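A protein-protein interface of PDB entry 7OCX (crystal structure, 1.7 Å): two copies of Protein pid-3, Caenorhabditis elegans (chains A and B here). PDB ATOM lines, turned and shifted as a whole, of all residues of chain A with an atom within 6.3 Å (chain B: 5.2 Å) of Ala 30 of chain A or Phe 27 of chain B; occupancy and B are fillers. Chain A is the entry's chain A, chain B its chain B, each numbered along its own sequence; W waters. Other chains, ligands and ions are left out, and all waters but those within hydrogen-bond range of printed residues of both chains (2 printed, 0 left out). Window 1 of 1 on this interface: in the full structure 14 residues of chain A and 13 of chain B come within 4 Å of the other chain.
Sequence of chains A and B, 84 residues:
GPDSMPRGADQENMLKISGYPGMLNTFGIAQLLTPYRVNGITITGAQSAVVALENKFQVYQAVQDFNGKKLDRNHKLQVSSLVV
The backbone carbonyl oxygen of Ala 30 of chain B sits at hydrogen-bond distance from the side-chain amide nitrogen of Gln 31 of chain A.
The backbone carbonyl oxygen of Ala 30 of chain A sits at hydrogen-bond distance from the side-chain amide nitrogen of Gln 31 of chain B (3.0 Å).
The side-chain amide oxygen (OD1) of Asn 39 of chain A sits at hydrogen-bond distance from the side-chain amide nitrogen (ND2) of Asn 25 of chain B, at 3.3 Å.
The backbone carbonyl oxygen (O) of Tyr 36 of chain A lies within hydrogen-bond range of the side-chain amide nitrogen (NE2) of Gln 31 of chain B.
The backbone carbonyl oxygen of Val 38 of chain A lies within hydrogen-bond range of the side-chain amide nitrogen of Asn 25 of chain B (2.8 Å).
OD1 of Asn 25 of chain B sits at hydrogen-bond distance from N of Phe 27 of chain B (3.1 Å).
OG1 of Thr 34 of chain A is in hydrogen-bond range of O of Gln 31 of chain A, 2.8 Å away.
The backbone NH (N) of Gly 28 of chain B lies within hydrogen-bond range of the side-chain amide oxygen (OD1) of Asn 25 of chain B, at 2.9 Å.
The side-chain amide oxygen (OD1) of Asn 25 of chain A is in hydrogen-bond range of the backbone NH (N) of Phe 27 of chain A (3.1 Å).
Among the printed residues, merely in contact across the chains: Thr 26 of chain A with Phe 27 of chain B, Phe 27 of chain A with Ala 30 of chain B, Ala 30 of chain A with Phe 27 of chain B, Leu 33 of chain A with Gln 31 of chain B, Thr 34 of chain A with Gln 31 of chain B, Val 38 of chain A with Phe 27 of chain B, Val 38 of chain A with Gln 31 of chain B, Asn 39 of chain A with Phe 27 of chain B, Gly 40 of chain A with Phe 27 of chain B and Ile 41 of chain A with Phe 27 of chain B.
Of chain B, only Phe 27 and Gln 31 come within 4 Å of Ala 30 of chain A.
Of the printed residues of chain A, Phe 27 of chain B touches Thr 26 (3.9 Å), Ala 30 (3.6 Å), Val 38 (3.4 Å), Asn 39 (3.99 Å), Gly 40 (3.9 Å) and Ile 41 (3.96 Å).
Of the printed residues of chain A, Ala 30 of chain B touches Phe 27 and Gln 31.
Of the printed residues of chain B, Tyr 36 of chain A touches Gln 31.
Printed residues of chain B within 4 Å of Asn 39 of chain A: Asn 25 (3.3 Å) and Phe 27 (3.99 Å).
Gly 28 of chain A touches none of the printed residues of chain B.
The nearest printed residue of chain A that does not touch Phe 27 of chain B is Phe 27 of chain A (4.05 Å).
Of the 15 printed residues of chain A, 11 touch a printed residue of chain B.
Hydrophobic or aromatic side chains of chain B that line the printed part of chain A: Phe 27 and Ala 30.
Thr 26 of chain A touches Phe 27 of chain B, but with the chains exchanged Phe 27 of chain A does not touch Thr 26 of chain B (4.1 Å).
Phe 27 of chain A touches Ala 30 of chain B, and with the chains exchanged Ala 30 of chain A touches Phe 27 of chain B.
Ala 30 of chain A touches Gln 31 of chain B, and with the chains exchanged Gln 31 of chain A touches Ala 30 of chain B.
Of the 15 pairs that touch across the chains among the printed residues, 4 have their exchanged pair printed and touching as well.
Water W2 lies within hydrogen-bond range of N of Val 38 of chain A (2.9 Å), OD1 of Asn 25 of chain B (3.2 Å), OE1 of Gln 31 of chain B (3.2 Å) and N of Gly 28 of chain B (3.3 Å).
Water W1 bridges ND2 of Asn 25 of chain B and OD1 of Asn 39 of chain A.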
ATOM      1  N   ASN A  25     -15.508  -4.604  -1.891  1.00  0.00           N
ATOM      2  CA  ASN A  25     -16.052  -4.393  -0.554  1.00  0.00           C
ATOM      3  C   ASN A  25     -17.559  -4.678  -0.588  1.00  0.00           C
ATOM      4  O   ASN A  25     -18.101  -5.111  -1.598  1.00  0.00           O
ATOM      5  CB  ASN A  25     -15.738  -2.981  -0.047  1.00  0.00           C
ATOM      6  CG  ASN A  25     -16.319  -1.860  -0.908  1.00  0.00           C
ATOM      7  OD1 ASN A  25     -17.236  -2.048  -1.698  1.00  0.00           O
ATOM      8  ND2 ASN A  25     -15.780  -0.662  -0.717  1.00  0.00           N
ATOM      9  N   THR A  26     -18.250  -4.451   0.537  1.00  0.00           N
ATOM     10  CA  THR A  26     -19.665  -4.826   0.541  1.00  0.00           C
ATOM     11  C   THR A  26     -20.482  -3.982  -0.417  1.00  0.00           C
ATOM     12  O   THR A  26     -21.443  -4.478  -1.008  1.00  0.00           O
ATOM     13  CB  THR A  26     -20.265  -4.740   1.951  1.00  0.00           C
ATOM     14  OG1 THR A  26     -20.077  -3.430   2.482  1.00  0.00           O
ATOM     15  CG2 THR A  26     -19.628  -5.772   2.871  1.00  0.00           C
ATOM     16  N   PHE A  27     -20.118  -2.712  -0.626  1.00  0.00           N
ATOM     17  CA  PHE A  27     -20.867  -1.965  -1.618  1.00  0.00           C
ATOM     18  C   PHE A  27     -20.678  -2.538  -3.019  1.00  0.00           C
ATOM     19  O   PHE A  27     -21.623  -2.562  -3.815  1.00  0.00           O
ATOM     20  CB  PHE A  27     -20.421  -0.525  -1.606  1.00  0.00           C
ATOM     21  CG  PHE A  27     -20.793   0.220  -0.373  1.00  0.00           C
ATOM     22  CD1 PHE A  27     -22.122   0.423  -0.027  1.00  0.00           C
ATOM     23  CD2 PHE A  27     -19.811   0.790   0.401  1.00  0.00           C
ATOM     24  CE1 PHE A  27     -22.447   1.193   1.091  1.00  0.00           C
ATOM     25  CE2 PHE A  27     -20.135   1.539   1.516  1.00  0.00           C
ATOM     26  CZ  PHE A  27     -21.447   1.737   1.863  1.00  0.00           C
ATOM     27  N   GLY A  28     -19.478  -3.019  -3.328  1.00  0.00           N
ATOM     28  CA  GLY A  28     -19.255  -3.619  -4.629  1.00  0.00           C
ATOM     29  C   GLY A  28     -20.038  -4.904  -4.829  1.00  0.00           C
ATOM     30  O   GLY A  28     -20.499  -5.185  -5.942  1.00  0.00           O
ATOM     31  N   ILE A  29     -20.203  -5.697  -3.766  1.00  0.00           N
ATOM     32  CA  ILE A  29     -21.007  -6.919  -3.857  1.00  0.00           C
ATOM     33  C   ILE A  29     -22.458  -6.544  -4.108  1.00  0.00           C
ATOM     34  O   ILE A  29     -23.126  -7.134  -4.957  1.00  0.00           O
ATOM     35  CB  ILE A  29     -20.839  -7.740  -2.568  1.00  0.00           C
ATOM     36  CG1 ILE A  29     -19.382  -8.210  -2.440  1.00  0.00           C
ATOM     37  CG2 ILE A  29     -21.762  -8.969  -2.570  1.00  0.00           C
ATOM     38  CD1 ILE A  29     -18.981  -8.659  -1.032  1.00  0.00           C
ATOM     39  N   ALA A  30     -22.944  -5.504  -3.432  1.00  0.00           N
ATOM     40  CA  ALA A  30     -24.300  -5.039  -3.694  1.00  0.00           C
ATOM     41  C   ALA A  30     -24.446  -4.564  -5.134  1.00  0.00           C
ATOM     42  O   ALA A  30     -25.492  -4.773  -5.760  1.00  0.00           O
ATOM     43  CB  ALA A  30     -24.663  -3.932  -2.716  1.00  0.00           C
ATOM     44  N   GLN A  31     -23.407  -3.945  -5.682  1.00  0.00           N
ATOM     45  CA  GLN A  31     -23.472  -3.504  -7.069  1.00  0.00           C
ATOM     46  C   GLN A  31     -23.629  -4.678  -8.022  1.00  0.00           C
ATOM     47  O   GLN A  31     -24.254  -4.520  -9.079  1.00  0.00           O
ATOM     48  CB  GLN A  31     -22.225  -2.666  -7.362  1.00  0.00           C
ATOM     49  CG  GLN A  31     -22.318  -1.261  -6.826  1.00  0.00           C
ATOM     50  CD  GLN A  31     -21.009  -0.497  -6.935  1.00  0.00           C
ATOM     51  OE1 GLN A  31     -19.939  -1.100  -6.964  1.00  0.00           O
ATOM     52  NE2 GLN A  31     -21.091   0.818  -7.089  1.00  0.00           N
ATOM     53  N   LEU A  32     -23.097  -5.851  -7.671  1.00  0.00           N
ATOM     54  CA  LEU A  32     -23.274  -7.024  -8.524  1.00  0.00           C
ATOM     55  C   LEU A  32     -24.722  -7.438  -8.643  1.00  0.00           C
ATOM     56  O   LEU A  32     -25.115  -8.076  -9.633  1.00  0.00           O
ATOM     57  CB  LEU A  32     -22.514  -8.219  -7.991  1.00  0.00           C
ATOM     58  CG  LEU A  32     -21.010  -8.125  -7.850  1.00  0.00           C
ATOM     59  CD1 LEU A  32     -20.566  -9.337  -7.073  1.00  0.00           C
ATOM     60  CD2 LEU A  32     -20.368  -8.009  -9.183  1.00  0.00           C
ATOM     61  N   LEU A  33     -25.509  -7.129  -7.633  1.00  0.00           N
ATOM     62  CA  LEU A  33     -26.875  -7.599  -7.505  1.00  0.00           C
ATOM     63  C   LEU A  33     -27.896  -6.566  -7.929  1.00  0.00           C
ATOM     64  O   LEU A  33     -29.103  -6.805  -7.751  1.00  0.00           O
ATOM     65  CB  LEU A  33     -27.135  -8.024  -6.063  1.00  0.00           C
ATOM     66  CG  LEU A  33     -26.282  -9.203  -5.608  1.00  0.00           C
ATOM     67  CD1 LEU A  33     -26.347  -9.400  -4.087  1.00  0.00           C
ATOM     68  CD2 LEU A  33     -26.723 -10.506  -6.255  1.00  0.00           C
ATOM     69  N   THR A  34     -27.460  -5.437  -8.488  1.00  0.00           N
ATOM     70  CA  THR A  34     -28.392  -4.464  -9.038  1.00  0.00           C
ATOM     71  C   THR A  34     -29.387  -5.169  -9.959  1.00  0.00           C
ATOM     72  O   THR A  34     -28.983  -5.998 -10.796  1.00  0.00           O
ATOM     73  CB  THR A  34     -27.638  -3.389  -9.825  1.00  0.00           C
ATOM     74  OG1 THR A  34     -26.593  -2.907  -8.990  1.00  0.00           O
ATOM     75  CG2 THR A  34     -28.558  -2.253 -10.239  1.00  0.00           C
ATOM     76  N   TYR A  36     -31.744  -5.520  -7.358  1.00  0.00           N
ATOM     77  CA  TYR A  36     -32.433  -6.106  -6.205  1.00  0.00           C
ATOM     78  C   TYR A  36     -32.054  -5.370  -4.930  1.00  0.00           C
ATOM     79  O   TYR A  36     -30.913  -4.932  -4.755  1.00  0.00           O
ATOM     80  CB  TYR A  36     -32.158  -7.630  -6.059  1.00  0.00           C
ATOM     81  CG  TYR A  36     -32.596  -8.327  -7.316  1.00  0.00           C
ATOM     82  CD1 TYR A  36     -33.950  -8.408  -7.628  1.00  0.00           C
ATOM     83  CD2 TYR A  36     -31.679  -8.804  -8.246  1.00  0.00           C
ATOM     84  CE1 TYR A  36     -34.373  -8.931  -8.847  1.00  0.00           C
ATOM     85  CE2 TYR A  36     -32.104  -9.371  -9.446  1.00  0.00           C
ATOM     86  CZ  TYR A  36     -33.450  -9.436  -9.735  1.00  0.00           C
ATOM     87  OH  TYR A  36     -33.867  -9.973 -10.913  1.00  0.00           O
ATOM     88  N   VAL A  38     -30.832  -4.836  -1.407  1.00  0.00           N
ATOM     89  CA  VAL A  38     -29.885  -5.466  -0.499  1.00  0.00           C
ATOM     90  C   VAL A  38     -30.002  -4.807   0.863  1.00  0.00           C
ATOM     91  O   VAL A  38     -29.808  -3.588   0.999  1.00  0.00           O
ATOM     92  CB  VAL A  38     -28.445  -5.338  -1.014  1.00  0.00           C
ATOM     93  CG1 VAL A  38     -27.451  -5.848   0.029  1.00  0.00           C
ATOM     94  CG2 VAL A  38     -28.254  -6.085  -2.299  1.00  0.00           C
ATOM     95  N   ASN A  39     -30.291  -5.611   1.885  1.00  0.00           N
ATOM     96  CA  ASN A  39     -30.438  -5.084   3.225  1.00  0.00           C
ATOM     97  C   ASN A  39     -29.245  -5.367   4.123  1.00  0.00           C
ATOM     98  O   ASN A  39     -29.052  -4.643   5.086  1.00  0.00           O
ATOM     99  CB  ASN A  39     -31.714  -5.626   3.880  1.00  0.00           C
ATOM    100  CG  ASN A  39     -32.962  -5.000   3.300  1.00  0.00           C
ATOM    101  OD1 ASN A  39     -32.958  -3.851   2.877  1.00  0.00           O
ATOM    102  ND2 ASN A  39     -34.041  -5.745   3.289  1.00  0.00           N
ATOM    103  N   GLY A  40     -28.425  -6.367   3.817  1.00  0.00           N
ATOM    104  CA  GLY A  40     -27.225  -6.589   4.600  1.00  0.00           C
ATOM    105  C   GLY A  40     -26.300  -7.526   3.868  1.00  0.00           C
ATOM    106  O   GLY A  40     -26.730  -8.361   3.068  1.00  0.00           O
ATOM    107  N   ILE A  41     -25.011  -7.387   4.163  1.00  0.00           N
ATOM    108  CA  ILE A  41     -24.018  -8.266   3.573  1.00  0.00           C
ATOM    109  C   ILE A  41     -23.018  -8.670   4.646  1.00  0.00           C
ATOM    110  O   ILE A  41     -22.539  -7.817   5.392  1.00  0.00           O
ATOM    111  CB  ILE A  41     -23.292  -7.614   2.377  1.00  0.00           C
ATOM    112  CG1 ILE A  41     -24.289  -7.251   1.268  1.00  0.00           C
ATOM    113  CG2 ILE A  41     -22.222  -8.584   1.856  1.00  0.00           C
ATOM    114  CD1 ILE A  41     -23.660  -6.692  -0.036  1.00  0.00           C
ATOM    115  N   ASN B  25     -31.769   2.527   0.564  1.00  0.00           N
ATOM    116  CA  ASN B  25     -30.818   2.434   1.656  1.00  0.00           C
ATOM    117  C   ASN B  25     -29.421   2.637   1.081  1.00  0.00           C
ATOM    118  O   ASN B  25     -29.236   2.865  -0.122  1.00  0.00           O
ATOM    119  CB  ASN B  25     -30.921   1.107   2.417  1.00  0.00           C
ATOM    120  CG  ASN B  25     -30.697  -0.104   1.531  1.00  0.00           C
ATOM    121  OD1 ASN B  25     -30.057  -0.007   0.481  1.00  0.00           O
ATOM    122  ND2 ASN B  25     -31.133  -1.275   2.004  1.00  0.00           N
ATOM    123  N   THR B  26     -28.410   2.537   1.942  1.00  0.00           N
ATOM    124  CA  THR B  26     -27.068   2.840   1.456  1.00  0.00           C
ATOM    125  C   THR B  26     -26.637   1.899   0.344  1.00  0.00           C
ATOM    126  O   THR B  26     -25.965   2.313  -0.602  1.00  0.00           O
ATOM    127  CB  THR B  26     -26.052   2.834   2.595  1.00  0.00           C
ATOM    128  OG1 THR B  26     -26.004   1.550   3.211  1.00  0.00           O
ATOM    129  CG2 THR B  26     -26.436   3.867   3.617  1.00  0.00           C
ATOM    130  N   PHE B  27     -26.993   0.612   0.435  1.00  0.00           N
ATOM    131  CA  PHE B  27     -26.624  -0.279  -0.639  1.00  0.00           C
ATOM    132  C   PHE B  27     -27.299   0.124  -1.943  1.00  0.00           C
ATOM    133  O   PHE B  27     -26.698   0.026  -3.019  1.00  0.00           O
ATOM    134  CB  PHE B  27     -27.015  -1.699  -0.261  1.00  0.00           C
ATOM    135  CG  PHE B  27     -26.172  -2.288   0.826  1.00  0.00           C
ATOM    136  CD1 PHE B  27     -24.834  -2.510   0.628  1.00  0.00           C
ATOM    137  CD2 PHE B  27     -26.720  -2.642   2.021  1.00  0.00           C
ATOM    138  CE1 PHE B  27     -24.065  -3.105   1.599  1.00  0.00           C
ATOM    139  CE2 PHE B  27     -25.946  -3.229   3.011  1.00  0.00           C
ATOM    140  CZ  PHE B  27     -24.619  -3.462   2.791  1.00  0.00           C
ATOM    141  N   GLY B  28     -28.540   0.593  -1.864  1.00  0.00           N
ATOM    142  CA  GLY B  28     -29.242   0.995  -3.069  1.00  0.00           C
ATOM    143  C   GLY B  28     -28.622   2.220  -3.718  1.00  0.00           C
ATOM    144  O   GLY B  28     -28.598   2.325  -4.948  1.00  0.00           O
ATOM    145  N   ILE B  29     -28.122   3.150  -2.903  1.00  0.00           N
ATOM    146  CA  ILE B  29     -27.402   4.314  -3.418  1.00  0.00           C
ATOM    147  C   ILE B  29     -26.125   3.858  -4.106  1.00  0.00           C
ATOM    148  O   ILE B  29     -25.806   4.301  -5.214  1.00  0.00           O
ATOM    149  CB  ILE B  29     -27.133   5.309  -2.273  1.00  0.00           C
ATOM    150  CG1 ILE B  29     -28.455   5.864  -1.719  1.00  0.00           C
ATOM    151  CG2 ILE B  29     -26.209   6.441  -2.752  1.00  0.00           C
ATOM    152  CD1 ILE B  29     -28.304   6.573  -0.420  1.00  0.00           C
ATOM    153  N   ALA B  30     -25.409   2.905  -3.505  1.00  0.00           N
ATOM    154  CA  ALA B  30     -24.228   2.359  -4.175  1.00  0.00           C
ATOM    155  C   ALA B  30     -24.584   1.719  -5.511  1.00  0.00           C
ATOM    156  O   ALA B  30     -23.814   1.815  -6.482  1.00  0.00           O
ATOM    157  CB  ALA B  30     -23.521   1.369  -3.254  1.00  0.00           C
ATOM    158  N   GLN B  31     -25.733   1.028  -5.582  1.00  0.00           N
ATOM    159  CA  GLN B  31     -26.162   0.402  -6.823  1.00  0.00           C
ATOM    160  C   GLN B  31     -26.405   1.442  -7.922  1.00  0.00           C
ATOM    161  O   GLN B  31     -26.149   1.171  -9.103  1.00  0.00           O
ATOM    162  CB  GLN B  31     -27.404  -0.467  -6.578  1.00  0.00           C
ATOM    163  CG  GLN B  31     -27.112  -1.719  -5.704  1.00  0.00           C
ATOM    164  CD  GLN B  31     -28.378  -2.488  -5.363  1.00  0.00           C
ATOM    165  OE1 GLN B  31     -29.388  -1.887  -5.006  1.00  0.00           O
ATOM    166  NE2 GLN B  31     -28.300  -3.817  -5.359  1.00  0.00           N
HETATM  167  O   HOH W   1     -32.414  -1.331   4.745  1.00  0.00           O
HETATM  168  O   HOH W   2     -30.431  -2.055  -1.937  1.00  0.00           O
